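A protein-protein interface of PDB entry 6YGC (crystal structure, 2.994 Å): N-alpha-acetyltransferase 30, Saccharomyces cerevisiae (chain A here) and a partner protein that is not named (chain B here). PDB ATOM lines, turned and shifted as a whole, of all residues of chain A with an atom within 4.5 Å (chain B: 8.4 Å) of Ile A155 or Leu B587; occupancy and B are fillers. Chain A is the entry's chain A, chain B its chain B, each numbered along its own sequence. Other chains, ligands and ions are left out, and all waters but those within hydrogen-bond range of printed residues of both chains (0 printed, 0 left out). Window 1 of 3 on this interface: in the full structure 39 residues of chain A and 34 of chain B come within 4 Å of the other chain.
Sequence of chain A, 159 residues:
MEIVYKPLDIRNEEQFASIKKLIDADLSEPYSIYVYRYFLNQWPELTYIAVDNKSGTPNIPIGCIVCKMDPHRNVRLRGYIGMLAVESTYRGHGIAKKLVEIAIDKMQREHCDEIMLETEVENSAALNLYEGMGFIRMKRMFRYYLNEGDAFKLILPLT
The backbone carbonyl oxygen of Pro A157 lies within hydrogen-bond range of the side-chain hydroxyl of Ser B579, at 2.8 Å.
The backbone NH (N) of Leu A156 is in hydrogen-bond range of the backbone carbonyl oxygen (O) of Ile A115, at 2.9 Å. O of Ile A136 is in hydrogen-bond range of N of Ile A155 (3.2 Å). O of Lys A153 sits at hydrogen-bond distance from N of Met A138. The guanidinium group (NH2) of Arg B588 lies within salt-bridge range of the side-chain carboxylate (OE1) of Glu B464 (2.7 Å). The side-chain amide oxygen (OD1) of Asn B580 sits at hydrogen-bond distance from the backbone NH (N) of Leu B583 (2.8 Å).
Among the printed residues, pairs that only touch across the chains: Met A138 with Leu B587 (3.4 Å), Ile A136 with Glu B464 (3.6 Å), Ile A155 with Leu B587 (3.6 Å), Ile A136 with Ile B584 (3.6 Å), Pro A157 with Leu B587 (3.7 Å), Pro A157 with Leu B583 (3.7 Å), Ile A136 with Arg B588 (3.7 Å), Leu A156 with Ser B579 (3.7 Å), Ile A136 with Leu B587 (3.9 Å) and Pro A157 with Ile B584 (3.9 Å).
Ile A115 touches none of the printed residues of chain B. Of the printed residues of chain B, Met A138 touches Leu B587 (3.4 Å). Of the printed residues of chain B, Pro A157 touches Ser B579, Leu B583, Ile B584 and Leu B587. Of the printed residues of chain A, Ser B579 touches Leu A156 and Pro A157. Arg B582 touches none of the printed residues of chain A. Leu B587 touches four residues of chain A. The nearest residue of chain B that does not touch Ile A155 is Ile B584 (6.3 Å). The nearest printed residue of chain A that does not touch Ile B584 is Leu A156 (4.8 Å).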
ATOM      1  N   ARG A  78       3.507   7.267 -35.133  1.00  0.00           N
ATOM      2  CA  ARG A  78       4.465   6.655 -34.218  1.00  0.00           C
ATOM      3  C   ARG A  78       4.506   5.154 -34.475  1.00  0.00           C
ATOM      4  O   ARG A  78       3.533   4.445 -34.197  1.00  0.00           O
ATOM      5  CB  ARG A  78       4.101   6.949 -32.764  1.00  0.00           C
ATOM      6  CG  ARG A  78       4.894   6.134 -31.757  1.00  0.00           C
ATOM      7  CD  ARG A  78       4.447   6.430 -30.334  1.00  0.00           C
ATOM      8  NE  ARG A  78       4.984   7.692 -29.831  1.00  0.00           N
ATOM      9  CZ  ARG A  78       4.666   8.223 -28.653  1.00  0.00           C
ATOM     10  NH1 ARG A  78       3.805   7.604 -27.854  1.00  0.00           N
ATOM     11  NH2 ARG A  78       5.206   9.373 -28.276  1.00  0.00           N
ATOM     12  N   GLU A 114       8.501   8.602 -35.859  1.00  0.00           N
ATOM     13  CA  GLU A 114       9.255   8.156 -34.697  1.00  0.00           C
ATOM     14  C   GLU A 114       8.979   6.679 -34.462  1.00  0.00           C
ATOM     15  O   GLU A 114       7.970   6.135 -34.922  1.00  0.00           O
ATOM     16  CB  GLU A 114       8.893   8.977 -33.454  1.00  0.00           C
ATOM     17  CG  GLU A 114       7.432   8.865 -33.045  1.00  0.00           C
ATOM     18  CD  GLU A 114       6.993   9.994 -32.135  1.00  0.00           C
ATOM     19  OE1 GLU A 114       7.635  11.066 -32.163  1.00  0.00           O
ATOM     20  OE2 GLU A 114       6.007   9.812 -31.392  1.00  0.00           O
ATOM     21  N   ILE A 115       9.895   6.038 -33.739  1.00  0.00           N
ATOM     22  CA  ILE A 115       9.747   4.656 -33.302  1.00  0.00           C
ATOM     23  C   ILE A 115       9.776   4.644 -31.780  1.00  0.00           C
ATOM     24  O   ILE A 115      10.655   5.261 -31.168  1.00  0.00           O
ATOM     25  CB  ILE A 115      10.853   3.750 -33.873  1.00  0.00           C
ATOM     26  CG1 ILE A 115      10.996   3.957 -35.382  1.00  0.00           C
ATOM     27  CG2 ILE A 115      10.555   2.290 -33.560  1.00  0.00           C
ATOM     28  CD1 ILE A 115       9.790   3.514 -36.173  1.00  0.00           C
ATOM     29  N   MET A 116       8.817   3.950 -31.173  1.00  0.00           N
ATOM     30  CA  MET A 116       8.698   3.886 -29.724  1.00  0.00           C
ATOM     31  C   MET A 116       8.684   2.433 -29.267  1.00  0.00           C
ATOM     32  O   MET A 116       8.230   1.543 -29.990  1.00  0.00           O
ATOM     33  CB  MET A 116       7.426   4.601 -29.237  1.00  0.00           C
ATOM     34  CG  MET A 116       7.384   4.862 -27.733  1.00  0.00           C
ATOM     35  SD  MET A 116       6.654   3.520 -26.771  1.00  0.00           S
ATOM     36  CE  MET A 116       4.908   3.837 -27.018  1.00  0.00           C
ATOM     37  N   PHE A 135      18.284   5.472 -30.236  1.00  0.00           N
ATOM     38  CA  PHE A 135      17.225   5.628 -29.248  1.00  0.00           C
ATOM     39  C   PHE A 135      17.749   6.329 -28.001  1.00  0.00           C
ATOM     40  O   PHE A 135      18.910   6.173 -27.614  1.00  0.00           O
ATOM     41  CB  PHE A 135      16.646   4.266 -28.861  1.00  0.00           C
ATOM     42  CG  PHE A 135      15.696   3.694 -29.872  1.00  0.00           C
ATOM     43  CD1 PHE A 135      16.168   3.016 -30.982  1.00  0.00           C
ATOM     44  CD2 PHE A 135      14.326   3.818 -29.700  1.00  0.00           C
ATOM     45  CE1 PHE A 135      15.292   2.480 -31.911  1.00  0.00           C
ATOM     46  CE2 PHE A 135      13.443   3.283 -30.625  1.00  0.00           C
ATOM     47  CZ  PHE A 135      13.927   2.614 -31.732  1.00  0.00           C
ATOM     48  N   ILE A 136      16.875   7.115 -27.369  1.00  0.00           N
ATOM     49  CA  ILE A 136      17.169   7.749 -26.091  1.00  0.00           C
ATOM     50  C   ILE A 136      16.001   7.507 -25.147  1.00  0.00           C
ATOM     51  O   ILE A 136      14.861   7.302 -25.568  1.00  0.00           O
ATOM     52  CB  ILE A 136      17.447   9.266 -26.219  1.00  0.00           C
ATOM     53  CG1 ILE A 136      16.271   9.976 -26.894  1.00  0.00           C
ATOM     54  CG2 ILE A 136      18.752   9.513 -26.962  1.00  0.00           C
ATOM     55  CD1 ILE A 136      16.387  11.487 -26.875  1.00  0.00           C
ATOM     56  N   MET A 138      13.184   8.452 -22.713  1.00  0.00           N
ATOM     57  CA  MET A 138      12.303   9.587 -22.489  1.00  0.00           C
ATOM     58  C   MET A 138      11.462   9.463 -21.228  1.00  0.00           C
ATOM     59  O   MET A 138      10.843  10.452 -20.820  1.00  0.00           O
ATOM     60  CB  MET A 138      11.370   9.783 -23.694  1.00  0.00           C
ATOM     61  CG  MET A 138      12.080  10.127 -24.993  1.00  0.00           C
ATOM     62  SD  MET A 138      13.075  11.626 -24.864  1.00  0.00           S
ATOM     63  CE  MET A 138      11.862  12.794 -24.249  1.00  0.00           C
ATOM     64  N   LYS A 153      11.019   4.020 -21.489  1.00  0.00           N
ATOM     65  CA  LYS A 153      10.323   4.331 -22.731  1.00  0.00           C
ATOM     66  C   LYS A 153      11.347   4.936 -23.679  1.00  0.00           C
ATOM     67  O   LYS A 153      11.889   6.010 -23.408  1.00  0.00           O
ATOM     68  CB  LYS A 153       9.161   5.285 -22.476  1.00  0.00           C
ATOM     69  CG  LYS A 153       8.142   5.346 -23.599  1.00  0.00           C
ATOM     70  CD  LYS A 153       7.096   6.421 -23.339  1.00  0.00           C
ATOM     71  CE  LYS A 153       5.938   6.323 -24.323  1.00  0.00           C
ATOM     72  NZ  LYS A 153       4.952   7.431 -24.162  1.00  0.00           N
ATOM     73  N   LEU A 154      11.632   4.237 -24.772  1.00  0.00           N
ATOM     74  CA  LEU A 154      12.642   4.652 -25.734  1.00  0.00           C
ATOM     75  C   LEU A 154      11.970   5.210 -26.979  1.00  0.00           C
ATOM     76  O   LEU A 154      10.974   4.656 -27.458  1.00  0.00           O
ATOM     77  CB  LEU A 154      13.550   3.481 -26.116  1.00  0.00           C
ATOM     78  CG  LEU A 154      14.211   2.714 -24.969  1.00  0.00           C
ATOM     79  CD1 LEU A 154      15.216   1.707 -25.505  1.00  0.00           C
ATOM     80  CD2 LEU A 154      14.874   3.668 -23.993  1.00  0.00           C
ATOM     81  N   ILE A 155      12.517   6.305 -27.502  1.00  0.00           N
ATOM     82  CA  ILE A 155      11.996   6.949 -28.702  1.00  0.00           C
ATOM     83  C   ILE A 155      13.159   7.272 -29.629  1.00  0.00           C
ATOM     84  O   ILE A 155      14.185   7.800 -29.186  1.00  0.00           O
ATOM     85  CB  ILE A 155      11.197   8.225 -28.375  1.00  0.00           C
ATOM     86  CG1 ILE A 155       9.961   7.887 -27.541  1.00  0.00           C
ATOM     87  CG2 ILE A 155      10.771   8.927 -29.654  1.00  0.00           C
ATOM     88  CD1 ILE A 155       9.013   9.050 -27.367  1.00  0.00           C
ATOM     89  N   LEU A 156      12.998   6.950 -30.910  1.00  0.00           N
ATOM     90  CA  LEU A 156      13.961   7.305 -31.953  1.00  0.00           C
ATOM     91  C   LEU A 156      13.283   8.243 -32.940  1.00  0.00           C
ATOM     92  O   LEU A 156      12.457   7.799 -33.757  1.00  0.00           O
ATOM     93  CB  LEU A 156      14.479   6.058 -32.668  1.00  0.00           C
ATOM     94  CG  LEU A 156      15.348   6.290 -33.906  1.00  0.00           C
ATOM     95  CD1 LEU A 156      16.711   6.841 -33.518  1.00  0.00           C
ATOM     96  CD2 LEU A 156      15.488   5.012 -34.722  1.00  0.00           C
ATOM     97  N   PRO A 157      13.584   9.541 -32.906  1.00  0.00           N
ATOM     98  CA  PRO A 157      12.915  10.476 -33.822  1.00  0.00           C
ATOM     99  C   PRO A 157      13.432  10.310 -35.244  1.00  0.00           C
ATOM    100  O   PRO A 157      14.641  10.249 -35.478  1.00  0.00           O
ATOM    101  CB  PRO A 157      13.270  11.850 -33.246  1.00  0.00           C
ATOM    102  CG  PRO A 157      14.570  11.630 -32.561  1.00  0.00           C
ATOM    103  CD  PRO A 157      14.543  10.223 -32.021  1.00  0.00           C
ATOM    104  N   GLU B 464      24.857  12.390 -23.215  1.00  0.00           N
ATOM    105  CA  GLU B 464      23.938  13.496 -22.985  1.00  0.00           C
ATOM    106  C   GLU B 464      24.220  14.240 -21.687  1.00  0.00           C
ATOM    107  O   GLU B 464      23.468  15.156 -21.341  1.00  0.00           O
ATOM    108  CB  GLU B 464      22.492  12.991 -22.970  1.00  0.00           C
ATOM    109  CG  GLU B 464      21.983  12.503 -24.314  1.00  0.00           C
ATOM    110  CD  GLU B 464      20.539  12.044 -24.255  1.00  0.00           C
ATOM    111  OE1 GLU B 464      20.186  11.305 -23.312  1.00  0.00           O
ATOM    112  OE2 GLU B 464      19.757  12.430 -25.151  1.00  0.00           O
ATOM    113  N   SER B 579      18.519   8.372 -37.779  1.00  0.00           N
ATOM    114  CA  SER B 579      18.263   9.700 -37.243  1.00  0.00           C
ATOM    115  C   SER B 579      19.521  10.559 -37.330  1.00  0.00           C
ATOM    116  O   SER B 579      20.548  10.153 -37.881  1.00  0.00           O
ATOM    117  CB  SER B 579      17.763   9.604 -35.801  1.00  0.00           C
ATOM    118  OG  SER B 579      17.385  10.879 -35.309  1.00  0.00           O
ATOM    119  N   ASN B 580      19.426  11.768 -36.779  1.00  0.00           N
ATOM    120  CA  ASN B 580      20.545  12.695 -36.708  1.00  0.00           C
ATOM    121  C   ASN B 580      20.606  13.301 -35.311  1.00  0.00           C
ATOM    122  O   ASN B 580      19.685  13.153 -34.503  1.00  0.00           O
ATOM    123  CB  ASN B 580      20.437  13.799 -37.771  1.00  0.00           C
ATOM    124  CG  ASN B 580      19.146  14.583 -37.670  1.00  0.00           C
ATOM    125  OD1 ASN B 580      19.007  15.467 -36.824  1.00  0.00           O
ATOM    126  ND2 ASN B 580      18.193  14.269 -38.540  1.00  0.00           N
ATOM    127  N   GLU B 581      21.714  13.994 -35.035  1.00  0.00           N
ATOM    128  CA  GLU B 581      21.927  14.553 -33.702  1.00  0.00           C
ATOM    129  C   GLU B 581      20.922  15.650 -33.388  1.00  0.00           C
ATOM    130  O   GLU B 581      20.466  15.773 -32.246  1.00  0.00           O
ATOM    131  CB  GLU B 581      23.345  15.102 -33.583  1.00  0.00           C
ATOM    132  CG  GLU B 581      24.291  14.617 -34.656  1.00  0.00           C
ATOM    133  CD  GLU B 581      25.590  15.390 -34.660  1.00  0.00           C
ATOM    134  OE1 GLU B 581      25.814  16.174 -33.714  1.00  0.00           O
ATOM    135  OE2 GLU B 581      26.385  15.218 -35.608  1.00  0.00           O
ATOM    136  N   ARG B 582      20.579  16.468 -34.386  1.00  0.00           N
ATOM    137  CA  ARG B 582      19.691  17.599 -34.141  1.00  0.00           C
ATOM    138  C   ARG B 582      18.298  17.131 -33.741  1.00  0.00           C
ATOM    139  O   ARG B 582      17.675  17.710 -32.844  1.00  0.00           O
ATOM    140  CB  ARG B 582      19.632  18.492 -35.382  1.00  0.00           C
ATOM    141  CG  ARG B 582      18.951  19.837 -35.157  1.00  0.00           C
ATOM    142  CD  ARG B 582      18.933  20.678 -36.432  1.00  0.00           C
ATOM    143  NE  ARG B 582      20.262  21.144 -36.822  1.00  0.00           N
ATOM    144  CZ  ARG B 582      20.726  22.369 -36.593  1.00  0.00           C
ATOM    145  NH1 ARG B 582      19.967  23.265 -35.976  1.00  0.00           N
ATOM    146  NH2 ARG B 582      21.948  22.704 -36.985  1.00  0.00           N
ATOM    147  N   LEU B 583      17.794  16.077 -34.390  1.00  0.00           N
ATOM    148  CA  LEU B 583      16.477  15.552 -34.041  1.00  0.00           C
ATOM    149  C   LEU B 583      16.473  14.939 -32.646  1.00  0.00           C
ATOM    150  O   LEU B 583      15.517  15.122 -31.883  1.00  0.00           O
ATOM    151  CB  LEU B 583      16.029  14.523 -35.079  1.00  0.00           C
ATOM    152  CG  LEU B 583      15.403  15.084 -36.355  1.00  0.00           C
ATOM    153  CD1 LEU B 583      15.107  13.963 -37.337  1.00  0.00           C
ATOM    154  CD2 LEU B 583      14.136  15.851 -36.016  1.00  0.00           C
ATOM    155  N   ILE B 584      17.534  14.208 -32.296  1.00  0.00           N
ATOM    156  CA  ILE B 584      17.614  13.600 -30.972  1.00  0.00           C
ATOM    157  C   ILE B 584      17.767  14.670 -29.896  1.00  0.00           C
ATOM    158  O   ILE B 584      17.205  14.552 -28.799  1.00  0.00           O
ATOM    159  CB  ILE B 584      18.765  12.577 -30.931  1.00  0.00           C
ATOM    160  CG1 ILE B 584      18.494  11.432 -31.910  1.00  0.00           C
ATOM    161  CG2 ILE B 584      18.962  12.043 -29.526  1.00  0.00           C
ATOM    162  CD1 ILE B 584      19.599  10.397 -31.959  1.00  0.00           C
ATOM    163  N   HIS B 585      18.517  15.734 -30.191  1.00  0.00           N
ATOM    164  CA  HIS B 585      18.703  16.797 -29.208  1.00  0.00           C
ATOM    165  C   HIS B 585      17.399  17.534 -28.931  1.00  0.00           C
ATOM    166  O   HIS B 585      17.086  17.838 -27.774  1.00  0.00           O
ATOM    167  CB  HIS B 585      19.779  17.773 -29.683  1.00  0.00           C
ATOM    168  CG  HIS B 585      19.916  18.986 -28.818  1.00  0.00           C
ATOM    169  ND1 HIS B 585      19.319  20.190 -29.126  1.00  0.00           N
ATOM    170  CD2 HIS B 585      20.574  19.178 -27.650  1.00  0.00           C
ATOM    171  CE1 HIS B 585      19.607  21.074 -28.186  1.00  0.00           C
ATOM    172  NE2 HIS B 585      20.367  20.485 -27.280  1.00  0.00           N
ATOM    173  N   ASN B 586      16.626  17.834 -29.978  1.00  0.00           N
ATOM    174  CA  ASN B 586      15.343  18.502 -29.778  1.00  0.00           C
ATOM    175  C   ASN B 586      14.391  17.628 -28.973  1.00  0.00           C
ATOM    176  O   ASN B 586      13.622  18.133 -28.146  1.00  0.00           O
ATOM    177  CB  ASN B 586      14.722  18.868 -31.125  1.00  0.00           C
ATOM    178  CG  ASN B 586      15.553  19.874 -31.896  1.00  0.00           C
ATOM    179  OD1 ASN B 586      16.336  20.626 -31.315  1.00  0.00           O
ATOM    180  ND2 ASN B 586      15.383  19.895 -33.213  1.00  0.00           N
ATOM    181  N   LEU B 587      14.430  16.313 -29.201  1.00  0.00           N
ATOM    182  CA  LEU B 587      13.558  15.405 -28.462  1.00  0.00           C
ATOM    183  C   LEU B 587      13.894  15.407 -26.976  1.00  0.00           C
ATOM    184  O   LEU B 587      12.993  15.380 -26.128  1.00  0.00           O
ATOM    185  CB  LEU B 587      13.668  13.995 -29.035  1.00  0.00           C
ATOM    186  CG  LEU B 587      12.820  12.924 -28.350  1.00  0.00           C
ATOM    187  CD1 LEU B 587      11.342  13.257 -28.472  1.00  0.00           C
ATOM    188  CD2 LEU B 587      13.116  11.561 -28.939  1.00  0.00           C
ATOM    189  N   ARG B 588      15.186  15.435 -26.642  1.00  0.00           N
ATOM    190  CA  ARG B 588      15.589  15.476 -25.240  1.00  0.00           C
ATOM    191  C   ARG B 588      15.065  16.730 -24.553  1.00  0.00           C
ATOM    192  O   ARG B 588      14.631  16.680 -23.396  1.00  0.00           O
ATOM    193  CB  ARG B 588      17.113  15.396 -25.131  1.00  0.00           C
ATOM    194  CG  ARG B 588      17.653  15.577 -23.720  1.00  0.00           C
ATOM    195  CD  ARG B 588      17.064  14.548 -22.771  1.00  0.00           C
ATOM    196  NE  ARG B 588      17.566  13.203 -23.032  1.00  0.00           N
ATOM    197  CZ  ARG B 588      16.985  12.093 -22.589  1.00  0.00           C
ATOM    198  NH1 ARG B 588      15.872  12.170 -21.874  1.00  0.00           N
ATOM    199  NH2 ARG B 588      17.510  10.908 -22.869  1.00  0.00           N
ATOM    200  N   PHE B 589      15.085  17.864 -25.254  1.00  0.00           N
ATOM    201  CA  PHE B 589      14.662  19.141 -24.696  1.00  0.00           C
ATOM    202  C   PHE B 589      13.256  19.535 -25.137  1.00  0.00           C
ATOM    203  O   PHE B 589      12.928  20.725 -25.142  1.00  0.00           O
ATOM    204  CB  PHE B 589      15.665  20.233 -25.070  1.00  0.00           C
ATOM    205  CG  PHE B 589      17.022  20.044 -24.453  1.00  0.00           C
ATOM    206  CD1 PHE B 589      17.328  20.616 -23.230  1.00  0.00           C
ATOM    207  CD2 PHE B 589      17.990  19.289 -25.094  1.00  0.00           C
ATOM    208  CE1 PHE B 589      18.576  20.440 -22.658  1.00  0.00           C
ATOM    209  CE2 PHE B 589      19.238  19.108 -24.528  1.00  0.00           C
ATOM    210  CZ  PHE B 589      19.532  19.685 -23.309  1.00  0.00           C
ATOM    211  N   LYS B 590      12.424  18.561 -25.502  1.00  0.00           N
ATOM    212  CA  LYS B 590      11.053  18.869 -25.900  1.00  0.00           C
ATOM    213  C   LYS B 590      10.234  19.551 -24.807  1.00  0.00           C
ATOM    214  O   LYS B 590       9.507  20.506 -25.135  1.00  0.00           O
ATOM    215  CB  LYS B 590      10.349  17.591 -26.377  1.00  0.00           C
ATOM    216  CG  LYS B 590       8.930  17.818 -26.877  1.00  0.00           C
ATOM    217  CD  LYS B 590       8.254  16.509 -27.246  1.00  0.00           C
ATOM    218  CE  LYS B 590       8.133  15.594 -26.038  1.00  0.00           C
ATOM    219  NZ  LYS B 590       7.292  16.188 -24.964  1.00  0.00           N
ATOM    220  N   PRO B 591      10.276  19.136 -23.535  1.00  0.00           N
ATOM    221  CA  PRO B 591       9.442  19.821 -22.530  1.00  0.00           C
ATOM    222  C   PRO B 591       9.766  21.297 -22.359  1.00  0.00           C
ATOM    223  O   PRO B 591       8.867  22.077 -22.020  1.00  0.00           O
ATOM    224  CB  PRO B 591       9.720  19.030 -21.242  1.00  0.00           C
ATOM    225  CG  PRO B 591      10.990  18.291 -21.501  1.00  0.00           C
ATOM    226  CD  PRO B 591      10.953  17.962 -22.953  1.00  0.00           C
ATOM    227  N   PHE B 592      11.010  21.709 -22.583  1.00  0.00           N
ATOM    228  CA  PHE B 592      11.408  23.101 -22.419  1.00  0.00           C
ATOM    229  C   PHE B 592      11.215  23.926 -23.686  1.00  0.00           C
ATOM    230  O   PHE B 592      11.751  25.035 -23.776  1.00  0.00           O
ATOM    231  CB  PHE B 592      12.871  23.185 -21.974  1.00  0.00           C
ATOM    232  CG  PHE B 592      13.276  22.108 -21.010  1.00  0.00           C
ATOM    233  CD1 PHE B 592      12.970  22.210 -19.663  1.00  0.00           C
ATOM    234  CD2 PHE B 592      13.972  20.995 -21.452  1.00  0.00           C
ATOM    235  CE1 PHE B 592      13.346  21.217 -18.774  1.00  0.00           C
ATOM    236  CE2 PHE B 592      14.350  19.999 -20.570  1.00  0.00           C
ATOM    237  CZ  PHE B 592      14.037  20.111 -19.229  1.00  0.00           C
ATOM    238  N   ASN B 593      10.458  23.417 -24.659  1.00  0.00           N
ATOM    239  CA  ASN B 593      10.372  24.073 -25.960  1.00  0.00           C
ATOM    240  C   ASN B 593       9.405  25.252 -25.944  1.00  0.00           C
ATOM    241  O   ASN B 593       9.664  26.275 -26.586  1.00  0.00           O
ATOM    242  CB  ASN B 593       9.957  23.059 -27.027  1.00  0.00           C
ATOM    243  CG  ASN B 593      10.821  23.134 -28.267  1.00  0.00           C
ATOM    244  OD1 ASN B 593      11.245  24.214 -28.679  1.00  0.00           O
ATOM    245  ND2 ASN B 593      11.093  21.981 -28.869  1.00  0.00           N
ATOM    246  N   LEU B 600      15.024  28.437 -24.337  1.00  0.00           N
ATOM    247  CA  LEU B 600      15.844  27.256 -24.572  1.00  0.00           C
ATOM    248  C   LEU B 600      16.943  27.593 -25.570  1.00  0.00           C
ATOM    249  O   LEU B 600      16.639  28.043 -26.683  1.00  0.00           O
ATOM    250  CB  LEU B 600      14.983  26.108 -25.092  1.00  0.00           C
ATOM    251  CG  LEU B 600      15.724  24.864 -25.583  1.00  0.00           C
ATOM    252  CD1 LEU B 600      16.522  24.227 -24.458  1.00  0.00           C
ATOM    253  CD2 LEU B 600      14.751  23.861 -26.185  1.00  0.00           C
